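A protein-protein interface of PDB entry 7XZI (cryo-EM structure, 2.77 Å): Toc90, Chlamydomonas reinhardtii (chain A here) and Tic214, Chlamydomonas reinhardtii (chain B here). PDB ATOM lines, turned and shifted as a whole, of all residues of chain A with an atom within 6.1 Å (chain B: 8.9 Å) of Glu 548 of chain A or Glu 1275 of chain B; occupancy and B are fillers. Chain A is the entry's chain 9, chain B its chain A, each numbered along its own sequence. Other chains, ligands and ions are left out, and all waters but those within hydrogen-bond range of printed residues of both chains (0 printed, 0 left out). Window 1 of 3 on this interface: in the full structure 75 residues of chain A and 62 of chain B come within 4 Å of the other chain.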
ATOM      1  N   LYS A 546      19.479  -1.801   8.550  1.00  0.00           N
ATOM      2  CA  LYS A 546      19.325  -0.415   8.124  1.00  0.00           C
ATOM      3  C   LYS A 546      20.679   0.283   8.124  1.00  0.00           C
ATOM      4  O   LYS A 546      21.309   0.425   9.181  1.00  0.00           O
ATOM      5  CB  LYS A 546      18.347   0.335   9.029  1.00  0.00           C
ATOM      6  CG  LYS A 546      18.170   1.799   8.645  1.00  0.00           C
ATOM      7  CD  LYS A 546      17.307   2.545   9.649  1.00  0.00           C
ATOM      8  CE  LYS A 546      17.116   3.998   9.238  1.00  0.00           C
ATOM      9  NZ  LYS A 546      18.414   4.717   9.096  1.00  0.00           N
ATOM     10  N   PRO A 547      21.158   0.730   6.967  1.00  0.00           N
ATOM     11  CA  PRO A 547      22.454   1.412   6.913  1.00  0.00           C
ATOM     12  C   PRO A 547      22.392   2.794   7.546  1.00  0.00           C
ATOM     13  O   PRO A 547      21.333   3.414   7.662  1.00  0.00           O
ATOM     14  CB  PRO A 547      22.744   1.501   5.413  1.00  0.00           C
ATOM     15  CG  PRO A 547      21.392   1.502   4.783  1.00  0.00           C
ATOM     16  CD  PRO A 547      20.520   0.638   5.643  1.00  0.00           C
ATOM     17  N   GLU A 548      23.564   3.275   7.959  1.00  0.00           N
ATOM     18  CA  GLU A 548      23.667   4.573   8.612  1.00  0.00           C
ATOM     19  C   GLU A 548      23.545   5.701   7.594  1.00  0.00           C
ATOM     20  O   GLU A 548      24.073   5.615   6.482  1.00  0.00           O
ATOM     21  CB  GLU A 548      24.994   4.686   9.363  1.00  0.00           C
ATOM     22  CG  GLU A 548      25.162   5.976  10.152  1.00  0.00           C
ATOM     23  CD  GLU A 548      24.195   6.082  11.316  1.00  0.00           C
ATOM     24  OE1 GLU A 548      23.721   5.031  11.798  1.00  0.00           O
ATOM     25  OE2 GLU A 548      23.908   7.218  11.750  1.00  0.00           O
ATOM     26  N   GLY A 549      22.847   6.763   7.985  1.00  0.00           N
ATOM     27  CA  GLY A 549      22.639   7.917   7.136  1.00  0.00           C
ATOM     28  C   GLY A 549      23.660   9.012   7.366  1.00  0.00           C
ATOM     29  O   GLY A 549      24.746   8.790   7.908  1.00  0.00           O
ATOM     30  N   TRP A 550      23.296  10.218   6.942  1.00  0.00           N
ATOM     31  CA  TRP A 550      24.163  11.380   7.062  1.00  0.00           C
ATOM     32  C   TRP A 550      24.093  11.977   8.465  1.00  0.00           C
ATOM     33  O   TRP A 550      23.161  11.725   9.235  1.00  0.00           O
ATOM     34  CB  TRP A 550      23.783  12.442   6.031  1.00  0.00           C
ATOM     35  CG  TRP A 550      24.272  12.151   4.651  1.00  0.00           C
ATOM     36  CD1 TRP A 550      25.480  11.623   4.306  1.00  0.00           C
ATOM     37  CD2 TRP A 550      23.561  12.365   3.427  1.00  0.00           C
ATOM     38  NE1 TRP A 550      25.569  11.499   2.941  1.00  0.00           N
ATOM     39  CE2 TRP A 550      24.403  11.947   2.378  1.00  0.00           C
ATOM     40  CE3 TRP A 550      22.295  12.869   3.115  1.00  0.00           C
ATOM     41  CZ2 TRP A 550      24.021  12.019   1.040  1.00  0.00           C
ATOM     42  CZ3 TRP A 550      21.917  12.940   1.787  1.00  0.00           C
ATOM     43  CH2 TRP A 550      22.777  12.517   0.766  1.00  0.00           C
ATOM     44  N   PRO A 698      29.546   8.716   4.494  1.00  0.00           N
ATOM     45  CA  PRO A 698      29.819   8.142   5.820  1.00  0.00           C
ATOM     46  C   PRO A 698      30.813   6.994   5.730  1.00  0.00           C
ATOM     47  O   PRO A 698      30.690   6.105   4.881  1.00  0.00           O
ATOM     48  CB  PRO A 698      28.440   7.666   6.288  1.00  0.00           C
ATOM     49  CG  PRO A 698      27.469   8.501   5.520  1.00  0.00           C
ATOM     50  CD  PRO A 698      28.107   8.728   4.180  1.00  0.00           C
ATOM     51  N   ASP A 700      33.396   4.443   8.312  1.00  0.00           N
ATOM     52  CA  ASP A 700      33.800   3.961   9.626  1.00  0.00           C
ATOM     53  C   ASP A 700      34.962   2.989   9.482  1.00  0.00           C
ATOM     54  O   ASP A 700      35.020   2.216   8.522  1.00  0.00           O
ATOM     55  CB  ASP A 700      32.640   3.267  10.351  1.00  0.00           C
ATOM     56  CG  ASP A 700      31.443   4.173  10.540  1.00  0.00           C
ATOM     57  OD1 ASP A 700      31.614   5.409  10.492  1.00  0.00           O
ATOM     58  OD2 ASP A 700      30.327   3.647  10.742  1.00  0.00           O
ATOM     59  N   SER A 721      29.151   4.159   3.286  1.00  0.00           N
ATOM     60  CA  SER A 721      27.741   4.341   2.965  1.00  0.00           C
ATOM     61  C   SER A 721      27.584   5.239   1.744  1.00  0.00           C
ATOM     62  O   SER A 721      28.347   6.191   1.561  1.00  0.00           O
ATOM     63  CB  SER A 721      26.983   4.940   4.152  1.00  0.00           C
ATOM     64  OG  SER A 721      25.610   5.109   3.845  1.00  0.00           O
ATOM     65  N   VAL A 723      24.326   7.130  -0.632  1.00  0.00           N
ATOM     66  CA  VAL A 723      22.912   7.469  -0.735  1.00  0.00           C
ATOM     67  C   VAL A 723      22.631   7.902  -2.164  1.00  0.00           C
ATOM     68  O   VAL A 723      23.367   8.723  -2.724  1.00  0.00           O
ATOM     69  CB  VAL A 723      22.521   8.576   0.260  1.00  0.00           C
ATOM     70  CG1 VAL A 723      21.018   8.804   0.240  1.00  0.00           C
ATOM     71  CG2 VAL A 723      22.997   8.226   1.660  1.00  0.00           C
ATOM     72  N   ILE A 734      19.766   3.214  -0.586  1.00  0.00           N
ATOM     73  CA  ILE A 734      21.052   3.266   0.099  1.00  0.00           C
ATOM     74  C   ILE A 734      21.847   2.010  -0.231  1.00  0.00           C
ATOM     75  O   ILE A 734      21.288   0.924  -0.411  1.00  0.00           O
ATOM     76  CB  ILE A 734      20.896   3.425   1.629  1.00  0.00           C
ATOM     77  CG1 ILE A 734      19.853   4.494   1.960  1.00  0.00           C
ATOM     78  CG2 ILE A 734      22.224   3.810   2.261  1.00  0.00           C
ATOM     79  CD1 ILE A 734      19.718   4.780   3.439  1.00  0.00           C
ATOM     80  N   GLN A 736      25.429   0.017   1.158  1.00  0.00           N
ATOM     81  CA  GLN A 736      26.477  -0.076   2.164  1.00  0.00           C
ATOM     82  C   GLN A 736      27.494  -1.128   1.747  1.00  0.00           C
ATOM     83  O   GLN A 736      27.123  -2.252   1.391  1.00  0.00           O
ATOM     84  CB  GLN A 736      25.891  -0.415   3.537  1.00  0.00           C
ATOM     85  CG  GLN A 736      26.902  -0.360   4.670  1.00  0.00           C
ATOM     86  CD  GLN A 736      26.264  -0.584   6.027  1.00  0.00           C
ATOM     87  OE1 GLN A 736      26.904  -0.406   7.064  1.00  0.00           O
ATOM     88  NE2 GLN A 736      24.996  -0.977   6.028  1.00  0.00           N
ATOM     89  N   LYS B1246      16.233  -8.718  20.745  1.00  0.00           N
ATOM     90  CA  LYS B1246      17.675  -8.758  20.524  1.00  0.00           C
ATOM     91  C   LYS B1246      18.290 -10.004  21.152  1.00  0.00           C
ATOM     92  O   LYS B1246      19.091 -10.706  20.524  1.00  0.00           O
ATOM     93  CB  LYS B1246      18.324  -7.490  21.085  1.00  0.00           C
ATOM     94  CG  LYS B1246      19.826  -7.405  20.865  1.00  0.00           C
ATOM     95  CD  LYS B1246      20.166  -7.364  19.384  1.00  0.00           C
ATOM     96  CE  LYS B1246      21.659  -7.195  19.167  1.00  0.00           C
ATOM     97  NZ  LYS B1246      22.170  -5.938  19.780  1.00  0.00           N
ATOM     98  N   ALA B1267      31.487  -4.996  15.110  1.00  0.00           N
ATOM     99  CA  ALA B1267      30.542  -3.923  15.391  1.00  0.00           C
ATOM    100  C   ALA B1267      29.431  -3.817  14.354  1.00  0.00           C
ATOM    101  O   ALA B1267      28.602  -2.905  14.451  1.00  0.00           O
ATOM    102  CB  ALA B1267      31.280  -2.586  15.494  1.00  0.00           C
ATOM    103  N   LEU B1268      29.391  -4.710  13.367  1.00  0.00           N
ATOM    104  CA  LEU B1268      28.386  -4.648  12.306  1.00  0.00           C
ATOM    105  C   LEU B1268      27.060  -5.291  12.700  1.00  0.00           C
ATOM    106  O   LEU B1268      26.563  -6.178  12.002  1.00  0.00           O
ATOM    107  CB  LEU B1268      28.948  -5.294  11.042  1.00  0.00           C
ATOM    108  N   SER B1269      26.473  -4.860  13.816  1.00  0.00           N
ATOM    109  CA  SER B1269      25.141  -5.309  14.223  1.00  0.00           C
ATOM    110  C   SER B1269      24.116  -4.241  13.838  1.00  0.00           C
ATOM    111  O   SER B1269      23.553  -3.530  14.671  1.00  0.00           O
ATOM    112  CB  SER B1269      25.112  -5.609  15.716  1.00  0.00           C
ATOM    113  OG  SER B1269      26.031  -6.636  16.044  1.00  0.00           O
ATOM    114  N   LYS B1270      23.877  -4.145  12.530  1.00  0.00           N
ATOM    115  CA  LYS B1270      23.012  -3.104  11.993  1.00  0.00           C
ATOM    116  C   LYS B1270      21.543  -3.479  12.124  1.00  0.00           C
ATOM    117  O   LYS B1270      20.807  -3.463  11.132  1.00  0.00           O
ATOM    118  CB  LYS B1270      23.349  -2.831  10.522  1.00  0.00           C
ATOM    119  CG  LYS B1270      24.760  -2.324  10.275  1.00  0.00           C
ATOM    120  CD  LYS B1270      24.963  -0.938  10.861  1.00  0.00           C
ATOM    121  CE  LYS B1270      26.323  -0.374  10.489  1.00  0.00           C
ATOM    122  NZ  LYS B1270      27.433  -1.240  10.972  1.00  0.00           N
ATOM    123  N   LYS B1271      21.102  -3.811  13.335  1.00  0.00           N
ATOM    124  CA  LYS B1271      19.693  -4.111  13.553  1.00  0.00           C
ATOM    125  C   LYS B1271      18.855  -2.859  13.334  1.00  0.00           C
ATOM    126  O   LYS B1271      19.248  -1.758  13.731  1.00  0.00           O
ATOM    127  CB  LYS B1271      19.480  -4.659  14.964  1.00  0.00           C
ATOM    128  CG  LYS B1271      18.032  -4.993  15.290  1.00  0.00           C
ATOM    129  CD  LYS B1271      17.454  -5.981  14.291  1.00  0.00           C
ATOM    130  CE  LYS B1271      15.980  -6.237  14.558  1.00  0.00           C
ATOM    131  NZ  LYS B1271      15.377  -7.140  13.539  1.00  0.00           N
ATOM    132  N   VAL B1272      17.697  -3.030  12.692  1.00  0.00           N
ATOM    133  CA  VAL B1272      16.846  -1.885  12.381  1.00  0.00           C
ATOM    134  C   VAL B1272      16.350  -1.221  13.661  1.00  0.00           C
ATOM    135  O   VAL B1272      16.296   0.011  13.755  1.00  0.00           O
ATOM    136  CB  VAL B1272      15.681  -2.314  11.467  1.00  0.00           C
ATOM    137  CG1 VAL B1272      14.919  -3.488  12.073  1.00  0.00           C
ATOM    138  CG2 VAL B1272      14.749  -1.139  11.202  1.00  0.00           C
ATOM    139  N   GLU B1273      15.993  -2.022  14.667  1.00  0.00           N
ATOM    140  CA  GLU B1273      15.492  -1.467  15.921  1.00  0.00           C
ATOM    141  C   GLU B1273      16.555  -0.623  16.613  1.00  0.00           C
ATOM    142  O   GLU B1273      16.266   0.465  17.126  1.00  0.00           O
ATOM    143  CB  GLU B1273      15.014  -2.594  16.837  1.00  0.00           C
ATOM    144  CG  GLU B1273      13.895  -3.442  16.252  1.00  0.00           C
ATOM    145  CD  GLU B1273      12.589  -2.682  16.123  1.00  0.00           C
ATOM    146  OE1 GLU B1273      12.405  -1.681  16.847  1.00  0.00           O
ATOM    147  OE2 GLU B1273      11.744  -3.086  15.296  1.00  0.00           O
ATOM    148  N   THR B1274      17.796  -1.110  16.637  1.00  0.00           N
ATOM    149  CA  THR B1274      18.872  -0.374  17.294  1.00  0.00           C
ATOM    150  C   THR B1274      19.269   0.858  16.487  1.00  0.00           C
ATOM    151  O   THR B1274      19.469   1.943  17.045  1.00  0.00           O
ATOM    152  CB  THR B1274      20.077  -1.288  17.508  1.00  0.00           C
ATOM    153  OG1 THR B1274      20.562  -1.746  16.239  1.00  0.00           O
ATOM    154  CG2 THR B1274      19.691  -2.491  18.358  1.00  0.00           C
ATOM    155  N   GLU B1275      19.392   0.706  15.166  1.00  0.00           N
ATOM    156  CA  GLU B1275      19.853   1.807  14.329  1.00  0.00           C
ATOM    157  C   GLU B1275      18.787   2.872  14.109  1.00  0.00           C
ATOM    158  O   GLU B1275      19.124   3.987  13.693  1.00  0.00           O
ATOM    159  CB  GLU B1275      20.340   1.275  12.982  1.00  0.00           C
ATOM    160  CG  GLU B1275      21.577   0.400  13.078  1.00  0.00           C
ATOM    161  CD  GLU B1275      22.800   1.169  13.538  1.00  0.00           C
ATOM    162  OE1 GLU B1275      22.906   2.372  13.216  1.00  0.00           O
ATOM    163  OE2 GLU B1275      23.654   0.571  14.226  1.00  0.00           O
ATOM    164  N   LYS B1276      17.514   2.561  14.361  1.00  0.00           N
ATOM    165  CA  LYS B1276      16.459   3.549  14.164  1.00  0.00           C
ATOM    166  C   LYS B1276      16.608   4.721  15.128  1.00  0.00           C
ATOM    167  O   LYS B1276      16.496   5.886  14.730  1.00  0.00           O
ATOM    168  CB  LYS B1276      15.089   2.887  14.327  1.00  0.00           C
ATOM    169  CG  LYS B1276      13.916   3.820  14.080  1.00  0.00           C
ATOM    170  CD  LYS B1276      12.603   3.057  14.087  1.00  0.00           C
ATOM    171  CE  LYS B1276      12.439   2.259  15.369  1.00  0.00           C
ATOM    172  NZ  LYS B1276      11.216   1.411  15.344  1.00  0.00           N
ATOM    173  N   SER B1277      16.873   4.431  16.401  1.00  0.00           N
ATOM    174  CA  SER B1277      17.053   5.476  17.409  1.00  0.00           C
ATOM    175  C   SER B1277      18.535   5.824  17.558  1.00  0.00           C
ATOM    176  O   SER B1277      19.133   5.716  18.629  1.00  0.00           O
ATOM    177  CB  SER B1277      16.448   5.039  18.737  1.00  0.00           C
ATOM    178  OG  SER B1277      17.038   3.834  19.193  1.00  0.00           O
ATOM    179  N   ASN B1278      19.130   6.251  16.446  1.00  0.00           N
ATOM    180  CA  ASN B1278      20.539   6.623  16.399  1.00  0.00           C
ATOM    181  C   ASN B1278      20.670   7.961  15.690  1.00  0.00           C
ATOM    182  O   ASN B1278      20.274   8.090  14.527  1.00  0.00           O
ATOM    183  CB  ASN B1278      21.369   5.551  15.687  1.00  0.00           C
ATOM    184  N   LEU B1279      21.221   8.950  16.389  1.00  0.00           N
ATOM    185  CA  LEU B1279      21.430  10.287  15.848  1.00  0.00           C
ATOM    186  C   LEU B1279      22.895  10.670  15.998  1.00  0.00           C
ATOM    187  O   LEU B1279      23.479  10.492  17.071  1.00  0.00           O
ATOM    188  CB  LEU B1279      20.539  11.313  16.554  1.00  0.00           C
ATOM    189  N   TYR B1280      23.480  11.194  14.926  1.00  0.00           N
ATOM    190  CA  TYR B1280      24.869  11.630  14.917  1.00  0.00           C
ATOM    191  C   TYR B1280      24.951  13.084  14.464  1.00  0.00           C
ATOM    192  O   TYR B1280      24.025  13.624  13.853  1.00  0.00           O
ATOM    193  CB  TYR B1280      25.722  10.735  14.009  1.00  0.00           C
ATOM    194  CG  TYR B1280      25.731   9.280  14.421  1.00  0.00           C
ATOM    195  N   GLN B1281      26.078  13.720  14.775  1.00  0.00           N
ATOM    196  CA  GLN B1281      26.291  15.121  14.443  1.00  0.00           C
ATOM    197  C   GLN B1281      27.679  15.296  13.847  1.00  0.00           C
ATOM    198  O   GLN B1281      28.587  14.503  14.106  1.00  0.00           O
ATOM    199  CB  GLN B1281      26.135  16.028  15.671  1.00  0.00           C
ATOM    200  CG  GLN B1281      24.770  15.967  16.333  1.00  0.00           C
ATOM    201  CD  GLN B1281      24.641  16.941  17.488  1.00  0.00           C
ATOM    202  OE1 GLN B1281      25.428  17.880  17.612  1.00  0.00           O
ATOM    203  NE2 GLN B1281      23.649  16.722  18.341  1.00  0.00           N
ATOM    204  N   LYS B1350      32.910  13.687  13.044  1.00  0.00           N
ATOM    205  CA  LYS B1350      31.586  13.121  13.269  1.00  0.00           C
ATOM    206  C   LYS B1350      31.528  12.462  14.642  1.00  0.00           C
ATOM    207  O   LYS B1350      32.334  11.576  14.946  1.00  0.00           O
ATOM    208  CB  LYS B1350      31.250  12.107  12.176  1.00  0.00           C
ATOM    209  CG  LYS B1350      29.978  11.317  12.417  1.00  0.00           C
ATOM    210  CD  LYS B1350      29.686  10.394  11.246  1.00  0.00           C
ATOM    211  CE  LYS B1350      28.496   9.497  11.534  1.00  0.00           C
ATOM    212  NZ  LYS B1350      28.774   8.558  12.654  1.00  0.00           N
ATOM    213  N   ILE B1352      28.616  11.883  18.344  1.00  0.00           N
ATOM    214  CA  ILE B1352      27.318  12.078  18.977  1.00  0.00           C
ATOM    215  C   ILE B1352      27.396  13.270  19.922  1.00  0.00           C
ATOM    216  O   ILE B1352      28.423  13.520  20.563  1.00  0.00           O
ATOM    217  CB  ILE B1352      26.880  10.795  19.711  1.00  0.00           C
ATOM    218  CG1 ILE B1352      27.115   9.571  18.823  1.00  0.00           C
ATOM    219  CG2 ILE B1352      25.416  10.879  20.112  1.00  0.00           C
ATOM    220  CD1 ILE B1352      26.745   8.258  19.475  1.00  0.00           C
ATOM    221  N   ARG B1358      17.245   9.330  19.630  1.00  0.00           N
ATOM    222  CA  ARG B1358      16.372   9.984  18.663  1.00  0.00           C
ATOM    223  C   ARG B1358      14.990  10.256  19.240  1.00  0.00           C
ATOM    224  O   ARG B1358      14.317  11.193  18.799  1.00  0.00           O
ATOM    225  CB  ARG B1358      16.257   9.129  17.399  1.00  0.00           C
ATOM    226  CG  ARG B1358      15.449   9.758  16.273  1.00  0.00           C
ATOM    227  CD  ARG B1358      16.287  10.714  15.437  1.00  0.00           C
ATOM    228  NE  ARG B1358      17.192  10.002  14.545  1.00  0.00           N
ATOM    229  CZ  ARG B1358      17.944  10.584  13.615  1.00  0.00           C
ATOM    230  NH1 ARG B1358      17.927  11.894  13.433  1.00  0.00           N
ATOM    231  NH2 ARG B1358      18.728   9.830  12.851  1.00  0.00           N
ATOM    232  N   TYR B1359      14.561   9.468  20.224  1.00  0.00           N
ATOM    233  CA  TYR B1359      13.272   9.647  20.880  1.00  0.00           C
ATOM    234  C   TYR B1359      13.504  10.411  22.178  1.00  0.00           C
ATOM    235  O   TYR B1359      14.155   9.903  23.098  1.00  0.00           O
ATOM    236  CB  TYR B1359      12.602   8.300  21.143  1.00  0.00           C
ATOM    237  CG  TYR B1359      12.167   7.574  19.890  1.00  0.00           C
ATOM    238  CD1 TYR B1359      13.086   6.896  19.099  1.00  0.00           C
ATOM    239  CD2 TYR B1359      10.835   7.562  19.500  1.00  0.00           C
ATOM    240  CE1 TYR B1359      12.692   6.233  17.954  1.00  0.00           C
ATOM    241  CE2 TYR B1359      10.431   6.900  18.357  1.00  0.00           C
ATOM    242  CZ  TYR B1359      11.363   6.238  17.588  1.00  0.00           C
ATOM    243  OH  TYR B1359      10.966   5.578  16.449  1.00  0.00           O
ATOM    244  N   HIS B1451      13.411   0.543  27.823  1.00  0.00           N
ATOM    245  CA  HIS B1451      14.489   1.124  27.024  1.00  0.00           C
ATOM    246  C   HIS B1451      14.033   2.374  26.273  1.00  0.00           C
ATOM    247  O   HIS B1451      14.855   3.114  25.722  1.00  0.00           O
ATOM    248  CB  HIS B1451      15.058   0.062  26.070  1.00  0.00           C
ATOM    249  CG  HIS B1451      15.804   0.620  24.898  1.00  0.00           C
ATOM    250  ND1 HIS B1451      16.867   1.486  25.034  1.00  0.00           N
ATOM    251  CD2 HIS B1451      15.635   0.435  23.567  1.00  0.00           C
ATOM    252  CE1 HIS B1451      17.322   1.810  23.836  1.00  0.00           C
ATOM    253  NE2 HIS B1451      16.592   1.186  22.930  1.00  0.00           N
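Of the 21 printed residues of chain B, 3 touch a printed residue of chain A.
Hydrophobic or aromatic side chains of chain B that line the printed part of chain A: Tyr 1280.
Along chain B the printed residues that touch a printed residue of chain A span positions 1270 to 1280.
Among the printed residues, 5 pairs touch across the chains.
Among the printed residues, no Asp or Glu carboxylate lies within 4 Å of a Lys or Arg side-chain nitrogen of the other chain.
The backbone NH of Lys 546 of chain A is in hydrogen-bond range of the backbone carbonyl oxygen of Lys 1270 of chain B (3.3 Å).
OE1 of Glu 548 of chain A sits close to OE1 of Glu 1275 of chain B.
No residue of chain B comes within 4 Å of Pro 547 of chain A.
No residue of chain B comes within 4 Å of Gly 549 of chain A.
Pro 698 of chain A touches none of the printed residues of chain B.
Of the printed residues of chain B, Gln 736 of chain A touches Lys 1270 (3.5 Å).
Leu 1268 of chain B touches none of the printed residues of chain A.
Glu 1275 of chain B touches just these residues of chain A: Lys 546 (3.9 Å) and Glu 548 (3.1 Å).
Of the printed residues of chain A, Tyr 1280 of chain B touches Glu 548.
The backbone carbonyl oxygen of Glu 548 of chain A is in hydrogen-bond range of the side-chain hydroxyl of Ser 721 of chain A, at 3.1 Å.
O of Lys 546 of chain A touches CG of Glu 1275 of chain B (3.9 Å).
Glu 548 of chain A touches Tyr 1280 of chain B (OE2 to CG, 3.8 Å).
Gln 736 of chain A touches Lys 1270 of chain B.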
